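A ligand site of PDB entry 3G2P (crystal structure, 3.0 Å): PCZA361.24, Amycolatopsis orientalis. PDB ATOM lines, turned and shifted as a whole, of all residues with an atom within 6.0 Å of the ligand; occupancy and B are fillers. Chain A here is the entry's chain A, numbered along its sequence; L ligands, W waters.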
ATOM      1  N   ALA A  66      -2.662  40.651 -13.298  1.00  0.00           N
ATOM      2  CA  ALA A  66      -2.818  39.583 -14.290  1.00  0.00           C
ATOM      3  C   ALA A  66      -2.810  40.096 -15.752  1.00  0.00           C
ATOM      4  O   ALA A  66      -3.732  40.807 -16.180  1.00  0.00           O
ATOM      5  CB  ALA A  66      -4.095  38.758 -13.990  1.00  0.00           C
ATOM      6  N   GLU A  71      -1.364  34.909 -24.414  1.00  0.00           N
ATOM      7  CA  GLU A  71      -2.101  33.661 -24.271  1.00  0.00           C
ATOM      8  C   GLU A  71      -3.406  33.786 -25.027  1.00  0.00           C
ATOM      9  O   GLU A  71      -3.703  32.983 -25.882  1.00  0.00           O
ATOM     10  CB  GLU A  71      -2.327  33.311 -22.788  1.00  0.00           C
ATOM     11  CG  GLU A  71      -2.909  31.906 -22.527  1.00  0.00           C
ATOM     12  CD  GLU A  71      -3.203  31.652 -21.054  1.00  0.00           C
ATOM     13  OE1 GLU A  71      -2.815  32.476 -20.213  1.00  0.00           O
ATOM     14  OE2 GLU A  71      -3.821  30.614 -20.731  1.00  0.00           O
ATOM     15  N   GLU A  88     -16.081  31.017 -22.576  1.00  0.00           N
ATOM     16  CA  GLU A  88     -14.961  30.833 -21.704  1.00  0.00           C
ATOM     17  C   GLU A  88     -15.375  30.310 -20.326  1.00  0.00           C
ATOM     18  O   GLU A  88     -16.213  30.929 -19.623  1.00  0.00           O
ATOM     19  CB  GLU A  88     -14.170  32.108 -21.562  1.00  0.00           C
ATOM     20  CG  GLU A  88     -12.831  31.844 -20.908  1.00  0.00           C
ATOM     21  CD  GLU A  88     -12.194  33.085 -20.330  1.00  0.00           C
ATOM     22  OE1 GLU A  88     -12.606  34.210 -20.695  1.00  0.00           O
ATOM     23  OE2 GLU A  88     -11.270  32.920 -19.502  1.00  0.00           O
ATOM     24  N   LEU A  89     -14.794  29.176 -19.929  1.00  0.00           N
ATOM     25  CA  LEU A  89     -15.134  28.518 -18.672  1.00  0.00           C
ATOM     26  C   LEU A  89     -14.246  28.990 -17.538  1.00  0.00           C
ATOM     27  O   LEU A  89     -13.054  29.121 -17.713  1.00  0.00           O
ATOM     28  CB  LEU A  89     -15.027  26.989 -18.802  1.00  0.00           C
ATOM     29  CG  LEU A  89     -16.015  26.333 -19.799  1.00  0.00           C
ATOM     30  CD1 LEU A  89     -15.656  24.866 -20.053  1.00  0.00           C
ATOM     31  CD2 LEU A  89     -17.502  26.479 -19.416  1.00  0.00           C
ATOM     32  N   ALA A  90     -14.825  29.239 -16.381  1.00  0.00           N
ATOM     33  CA  ALA A  90     -14.057  29.722 -15.240  1.00  0.00           C
ATOM     34  C   ALA A  90     -13.234  30.931 -15.669  1.00  0.00           C
ATOM     35  O   ALA A  90     -12.014  30.929 -15.561  1.00  0.00           O
ATOM     36  CB  ALA A  90     -13.157  28.631 -14.721  1.00  0.00           C
ATOM     37  N   ALA A  91     -13.925  31.949 -16.152  1.00  0.00           N
ATOM     38  CA  ALA A  91     -13.289  33.104 -16.771  1.00  0.00           C
ATOM     39  C   ALA A  91     -12.636  33.973 -15.752  1.00  0.00           C
ATOM     40  O   ALA A  91     -12.045  34.971 -16.089  1.00  0.00           O
ATOM     41  CB  ALA A  91     -14.300  33.897 -17.581  1.00  0.00           C
ATOM     42  N   GLY A  92     -12.733  33.590 -14.497  1.00  0.00           N
ATOM     43  CA  GLY A  92     -12.093  34.342 -13.452  1.00  0.00           C
ATOM     44  C   GLY A  92     -12.480  35.781 -13.605  1.00  0.00           C
ATOM     45  O   GLY A  92     -13.674  36.091 -13.737  1.00  0.00           O
ATOM     46  N   MET A  93     -11.484  36.659 -13.639  1.00  0.00           N
ATOM     47  CA  MET A  93     -11.737  38.083 -13.610  1.00  0.00           C
ATOM     48  C   MET A  93     -11.617  38.755 -14.962  1.00  0.00           C
ATOM     49  O   MET A  93     -11.668  39.982 -15.059  1.00  0.00           O
ATOM     50  CB  MET A  93     -10.808  38.753 -12.626  1.00  0.00           C
ATOM     51  CG  MET A  93     -11.310  38.617 -11.220  1.00  0.00           C
ATOM     52  SD  MET A  93     -10.930  40.105 -10.284  1.00  0.00           S
ATOM     53  CE  MET A  93     -11.734  41.361 -11.273  1.00  0.00           C
ATOM     54  N   GLY A  94     -11.455  37.947 -16.012  1.00  0.00           N
ATOM     55  CA  GLY A  94     -11.379  38.458 -17.373  1.00  0.00           C
ATOM     56  C   GLY A  94      -9.985  38.631 -17.913  1.00  0.00           C
ATOM     57  O   GLY A  94      -9.802  39.253 -18.952  1.00  0.00           O
ATOM     58  N   ARG A  95      -8.992  38.063 -17.236  1.00  0.00           N
ATOM     59  CA  ARG A  95      -7.616  38.059 -17.740  1.00  0.00           C
ATOM     60  C   ARG A  95      -7.548  37.779 -19.245  1.00  0.00           C
ATOM     61  O   ARG A  95      -6.937  38.546 -19.966  1.00  0.00           O
ATOM     62  CB  ARG A  95      -6.752  37.058 -16.980  1.00  0.00           C
ATOM     63  CG  ARG A  95      -5.267  37.177 -17.282  1.00  0.00           C
ATOM     64  CD  ARG A  95      -4.442  36.200 -16.443  1.00  0.00           C
ATOM     65  NE  ARG A  95      -4.690  34.822 -16.841  1.00  0.00           N
ATOM     66  CZ  ARG A  95      -3.941  34.156 -17.709  1.00  0.00           C
ATOM     67  NH1 ARG A  95      -2.885  34.729 -18.262  1.00  0.00           N
ATOM     68  NH2 ARG A  95      -4.263  32.909 -18.017  1.00  0.00           N
ATOM     69  N   LEU A  96      -8.158  36.694 -19.711  1.00  0.00           N
ATOM     70  CA  LEU A  96      -8.267  36.430 -21.143  1.00  0.00           C
ATOM     71  C   LEU A  96      -9.544  37.011 -21.744  1.00  0.00           C
ATOM     72  O   LEU A  96      -9.570  37.355 -22.929  1.00  0.00           O
ATOM     73  CB  LEU A  96      -8.231  34.925 -21.423  1.00  0.00           C
ATOM     74  CG  LEU A  96      -7.239  33.972 -20.743  1.00  0.00           C
ATOM     75  CD1 LEU A  96      -7.606  32.535 -21.055  1.00  0.00           C
ATOM     76  CD2 LEU A  96      -5.794  34.234 -21.128  1.00  0.00           C
ATOM     77  N   LEU A 110     -18.202  32.166 -17.978  1.00  0.00           N
ATOM     78  CA  LEU A 110     -18.815  31.374 -16.885  1.00  0.00           C
ATOM     79  C   LEU A 110     -17.896  31.236 -15.674  1.00  0.00           C
ATOM     80  O   LEU A 110     -16.784  30.780 -15.817  1.00  0.00           O
ATOM     81  CB  LEU A 110     -19.244  29.973 -17.400  1.00  0.00           C
ATOM     82  CG  LEU A 110     -19.737  28.891 -16.417  1.00  0.00           C
ATOM     83  CD1 LEU A 110     -20.763  27.915 -16.992  1.00  0.00           C
ATOM     84  CD2 LEU A 110     -18.570  28.141 -15.848  1.00  0.00           C
ATOM     85  N   GLU A 111     -18.377  31.583 -14.487  1.00  0.00           N
ATOM     86  CA  GLU A 111     -17.518  31.608 -13.306  1.00  0.00           C
ATOM     87  C   GLU A 111     -18.262  31.035 -12.107  1.00  0.00           C
ATOM     88  O   GLU A 111     -19.461  31.163 -12.035  1.00  0.00           O
ATOM     89  CB  GLU A 111     -17.022  33.036 -13.052  1.00  0.00           C
ATOM     90  CG  GLU A 111     -16.290  33.293 -11.744  1.00  0.00           C
ATOM     91  CD  GLU A 111     -15.123  32.326 -11.472  1.00  0.00           C
ATOM     92  OE1 GLU A 111     -14.215  32.186 -12.331  1.00  0.00           O
ATOM     93  OE2 GLU A 111     -15.126  31.719 -10.369  1.00  0.00           O
ATOM     94  N   LEU A 112     -17.559  30.386 -11.177  1.00  0.00           N
ATOM     95  CA  LEU A 112     -18.256  29.754 -10.080  1.00  0.00           C
ATOM     96  C   LEU A 112     -18.356  30.661  -8.873  1.00  0.00           C
ATOM     97  O   LEU A 112     -19.350  30.633  -8.167  1.00  0.00           O
ATOM     98  CB  LEU A 112     -17.567  28.451  -9.666  1.00  0.00           C
ATOM     99  CG  LEU A 112     -18.047  27.702  -8.413  1.00  0.00           C
ATOM    100  CD1 LEU A 112     -19.322  26.921  -8.629  1.00  0.00           C
ATOM    101  CD2 LEU A 112     -16.957  26.789  -7.963  1.00  0.00           C
ATOM    102  N   SER A 113     -17.319  31.462  -8.651  1.00  0.00           N
ATOM    103  CA  SER A 113     -17.225  32.318  -7.482  1.00  0.00           C
ATOM    104  C   SER A 113     -18.102  33.529  -7.657  1.00  0.00           C
ATOM    105  O   SER A 113     -17.839  34.328  -8.557  1.00  0.00           O
ATOM    106  CB  SER A 113     -15.771  32.804  -7.309  1.00  0.00           C
ATOM    107  OG  SER A 113     -15.679  33.799  -6.295  1.00  0.00           O
ATOM    108  N   VAL A 116     -15.786  36.718  -7.322  1.00  0.00           N
ATOM    109  CA  VAL A 116     -15.069  36.980  -8.584  1.00  0.00           C
ATOM    110  C   VAL A 116     -16.044  37.478  -9.652  1.00  0.00           C
ATOM    111  O   VAL A 116     -15.787  38.453 -10.326  1.00  0.00           O
ATOM    112  CB  VAL A 116     -14.296  35.735  -9.101  1.00  0.00           C
ATOM    113  CG1 VAL A 116     -13.843  35.930 -10.547  1.00  0.00           C
ATOM    114  CG2 VAL A 116     -13.104  35.391  -8.174  1.00  0.00           C
ATOM    115  N   GLY A 140     -22.013  29.307 -12.675  1.00  0.00           N
ATOM    116  CA  GLY A 140     -21.959  27.931 -13.166  1.00  0.00           C
ATOM    117  C   GLY A 140     -20.787  27.133 -12.642  1.00  0.00           C
ATOM    118  O   GLY A 140     -19.735  27.676 -12.304  1.00  0.00           O
ATOM    119  N   ASP A 141     -20.992  25.820 -12.581  1.00  0.00           N
ATOM    120  CA  ASP A 141     -19.930  24.865 -12.285  1.00  0.00           C
ATOM    121  C   ASP A 141     -19.420  24.166 -13.572  1.00  0.00           C
ATOM    122  O   ASP A 141     -20.095  23.306 -14.134  1.00  0.00           O
ATOM    123  CB  ASP A 141     -20.430  23.838 -11.281  1.00  0.00           C
ATOM    124  CG  ASP A 141     -19.371  22.861 -10.864  1.00  0.00           C
ATOM    125  OD1 ASP A 141     -18.450  22.584 -11.683  1.00  0.00           O
ATOM    126  OD2 ASP A 141     -19.473  22.360  -9.720  1.00  0.00           O
ATOM    127  N   MET A 142     -18.215  24.530 -14.021  1.00  0.00           N
ATOM    128  CA  MET A 142     -17.671  24.006 -15.272  1.00  0.00           C
ATOM    129  C   MET A 142     -17.620  22.464 -15.313  1.00  0.00           C
ATOM    130  O   MET A 142     -17.522  21.878 -16.405  1.00  0.00           O
ATOM    131  CB  MET A 142     -16.289  24.619 -15.581  1.00  0.00           C
ATOM    132  CG  MET A 142     -15.239  24.436 -14.465  1.00  0.00           C
ATOM    133  SD  MET A 142     -13.560  24.914 -14.975  1.00  0.00           S
ATOM    134  CE  MET A 142     -12.706  25.208 -13.422  1.00  0.00           C
ATOM    135  N   SER A 143     -17.704  21.824 -14.137  1.00  0.00           N
ATOM    136  CA  SER A 143     -17.775  20.370 -14.131  1.00  0.00           C
ATOM    137  C   SER A 143     -19.207  19.814 -14.424  1.00  0.00           C
ATOM    138  O   SER A 143     -19.387  18.638 -14.789  1.00  0.00           O
ATOM    139  CB  SER A 143     -17.173  19.803 -12.843  1.00  0.00           C
ATOM    140  OG  SER A 143     -17.937  20.125 -11.702  1.00  0.00           O
ATOM    141  N   SER A 157      -8.606  27.954 -19.668  1.00  0.00           N
ATOM    142  CA  SER A 157      -7.185  28.278 -19.445  1.00  0.00           C
ATOM    143  C   SER A 157      -6.594  27.259 -18.470  1.00  0.00           C
ATOM    144  O   SER A 157      -7.342  26.679 -17.660  1.00  0.00           O
ATOM    145  CB  SER A 157      -7.007  29.717 -18.944  1.00  0.00           C
ATOM    146  OG  SER A 157      -6.941  29.781 -17.524  1.00  0.00           O
ATOM    147  N   GLY A 159      -4.851  27.488 -15.849  1.00  0.00           N
ATOM    148  CA  GLY A 159      -5.228  27.843 -14.484  1.00  0.00           C
ATOM    149  C   GLY A 159      -6.476  27.094 -14.058  1.00  0.00           C
ATOM    150  O   GLY A 159      -6.478  26.403 -13.048  1.00  0.00           O
ATOM    151  N   SER A 160      -7.537  27.212 -14.864  1.00  0.00           N
ATOM    152  CA  SER A 160      -8.846  26.696 -14.545  1.00  0.00           C
ATOM    153  C   SER A 160      -8.966  25.173 -14.555  1.00  0.00           C
ATOM    154  O   SER A 160      -9.406  24.595 -13.566  1.00  0.00           O
ATOM    155  CB  SER A 160      -9.859  27.295 -15.505  1.00  0.00           C
ATOM    156  OG  SER A 160      -9.688  28.689 -15.582  1.00  0.00           O
ATOM    157  N   GLU A 163      -7.989  23.249 -11.543  1.00  0.00           N
ATOM    158  CA  GLU A 163      -8.704  23.310 -10.295  1.00  0.00           C
ATOM    159  C   GLU A 163      -9.511  22.032 -10.053  1.00  0.00           C
ATOM    160  O   GLU A 163      -9.873  21.734  -8.912  1.00  0.00           O
ATOM    161  CB  GLU A 163      -9.580  24.535 -10.244  1.00  0.00           C
ATOM    162  CG  GLU A 163      -8.763  25.774 -10.400  1.00  0.00           C
ATOM    163  CD  GLU A 163      -8.950  26.732  -9.245  1.00  0.00           C
ATOM    164  OE1 GLU A 163     -10.070  26.831  -8.706  1.00  0.00           O
ATOM    165  OE2 GLU A 163      -7.976  27.409  -8.863  1.00  0.00           O
ATOM    166  N   LEU A 164      -9.752  21.266 -11.109  1.00  0.00           N
ATOM    167  CA  LEU A 164     -10.631  20.106 -11.067  1.00  0.00           C
ATOM    168  C   LEU A 164      -9.872  18.804 -10.811  1.00  0.00           C
ATOM    169  O   LEU A 164      -8.813  18.591 -11.396  1.00  0.00           O
ATOM    170  CB  LEU A 164     -11.429  20.015 -12.386  1.00  0.00           C
ATOM    171  CG  LEU A 164     -12.329  21.215 -12.784  1.00  0.00           C
ATOM    172  CD1 LEU A 164     -13.115  20.926 -14.064  1.00  0.00           C
ATOM    173  CD2 LEU A 164     -13.286  21.611 -11.664  1.00  0.00           C
ATOM    174  N   ASP A 168     -14.286  15.460 -11.630  1.00  0.00           N
ATOM    175  CA  ASP A 168     -14.852  16.662 -12.174  1.00  0.00           C
ATOM    176  C   ASP A 168     -14.326  16.917 -13.582  1.00  0.00           C
ATOM    177  O   ASP A 168     -15.047  17.470 -14.414  1.00  0.00           O
ATOM    178  CB  ASP A 168     -14.585  17.860 -11.272  1.00  0.00           C
ATOM    179  CG  ASP A 168     -15.141  17.677  -9.867  1.00  0.00           C
ATOM    180  OD1 ASP A 168     -15.911  16.722  -9.615  1.00  0.00           O
ATOM    181  OD2 ASP A 168     -14.792  18.497  -9.007  1.00  0.00           O
HETATM  182  N1  LIG L   1      -9.380  32.035 -17.061  1.00  0.00           N
HETATM  183  C1  LIG L   1      -8.871  33.006 -16.049  1.00  0.00           C
HETATM  184  C2  LIG L   1      -9.001  32.553 -14.599  1.00  0.00           C
HETATM  185  C3  LIG L   1      -8.471  31.157 -14.283  1.00  0.00           C
HETATM  186  S1  LIG L   1      -8.093  30.963 -12.517  1.00  0.00           S
HETATM  187  C4  LIG L   1      -7.421  33.381 -16.355  1.00  0.00           C
HETATM  188  O1  LIG L   1      -6.860  32.949 -17.389  1.00  0.00           O
HETATM  189  O2  LIG L   1      -6.794  34.108 -15.560  1.00  0.00           O
HETATM  190  C5  LIG L   1      -9.338  29.719 -12.076  1.00  0.00           C
HETATM  191  C6  LIG L   1     -10.753  30.245 -11.972  1.00  0.00           C
HETATM  192  O3  LIG L   1     -11.622  29.148 -11.981  1.00  0.00           O
HETATM  193  C7  LIG L   1     -11.015  30.968 -10.663  1.00  0.00           C
HETATM  194  O4  LIG L   1     -11.513  32.223 -11.018  1.00  0.00           O
HETATM  195  C8  LIG L   1     -12.064  30.139  -9.920  1.00  0.00           C
HETATM  196  O5  LIG L   1     -13.040  30.913  -9.265  1.00  0.00           O
HETATM  197  C9  LIG L   1     -12.676  29.332 -11.043  1.00  0.00           C
HETATM  198  N2  LIG L   1     -13.228  28.009 -10.687  1.00  0.00           N
HETATM  199  C10 LIG L   1     -12.688  27.075  -9.854  1.00  0.00           C
HETATM  200  N3  LIG L   1     -13.476  25.977  -9.822  1.00  0.00           N
HETATM  201  C11 LIG L   1     -14.514  26.191 -10.657  1.00  0.00           C
HETATM  202  C12 LIG L   1     -15.607  25.415 -11.012  1.00  0.00           C
HETATM  203  N4  LIG L   1     -15.752  24.197 -10.481  1.00  0.00           N
HETATM  204  N5  LIG L   1     -16.534  25.912 -11.922  1.00  0.00           N
HETATM  205  C13 LIG L   1     -16.389  27.166 -12.482  1.00  0.00           C
HETATM  206  N6  LIG L   1     -15.287  27.932 -12.122  1.00  0.00           N
HETATM  207  C14 LIG L   1     -14.366  27.464 -11.219  1.00  0.00           C
HETATM  208  O   HOH W   1     -14.059  23.454  -8.214  1.00  0.00           O
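The side-chain carboxylate (OE2) of Glu 111 lies within hydrogen-bond range of an oxygen (O5) of the ligand (2.5 Å).
An oxygen (O2) of the ligand is in salt-bridge range of the guanidinium group (NE) of Arg 95 (2.6 Å).
N of Met 142 lies within hydrogen-bond range of N5 of the ligand.
O1 of the ligand sits at hydrogen-bond distance from OG of Ser 157 (3.2 Å).
A nitrogen (N1) of the ligand lies within hydrogen-bond range of the backbone carbonyl oxygen (O) of Ala 90.
A nitrogen (N1) of the ligand lies within salt-bridge range of the side-chain carboxylate (OE2) of Glu 88 (3.2 Å).
The backbone NH (N) of Leu 112 lies close to a nitrogen (N6) of the ligand.
N4 of the ligand sits at hydrogen-bond distance from OD1 of Asp 141 (3.4 Å).
N of Gly 92 lies within hydrogen-bond range of OE1 of Glu 111.
The backbone carbonyl oxygen (O) of Glu 111 sits at hydrogen-bond distance from the backbone NH (N) of Gly 140 (3.2 Å).
The side-chain carboxylate of Glu 111 lies within hydrogen-bond range of the backbone NH of Ser 113, 2.8 Å away.
The side-chain hydroxyl (OG) of Ser 160 is in hydrogen-bond range of the backbone carbonyl oxygen (O) of Ala 90.
The backbone NH (N) of Ala 90 sits at hydrogen-bond distance from the backbone carbonyl oxygen (O) of Leu 110 (2.6 Å).
O of Glu 88 is in hydrogen-bond range of N of Leu 110, 2.9 Å away.
OD1 of Asp 141 is in hydrogen-bond range of OG of Ser 143 (2.5 Å).
The backbone NH (N) of Ala 91 sits at hydrogen-bond distance from the backbone carbonyl oxygen (O) of Leu 110, 3.1 Å away.
Residues that only touch the ligand: Ala 91 (3.7 Å), Gly 92 (3.3 Å), Leu 96 (3.5 Å), Ser 113 (3.9 Å), Gly 140 (3.4 Å), Ser 160 (3.0 Å), Glu 163 (2.9 Å) and Leu 164 (3.8 Å).
Hydrophobic or aromatic side chains that line the ligand: Ala 90, Leu 96, Leu 112, Met 142 and Leu 164.
16 residues have an atom within 4 Å of the ligand: Glu 88, Ala 90, Ala 91, Gly 92, Arg 95, Leu 96, Glu 111, Leu 112, Ser 113, Gly 140, Asp 141, Met 142, Ser 157, Ser 160, Glu 163 and Leu 164.
The nearest printed residue that does not touch the ligand is Leu 110 (4.1 Å).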
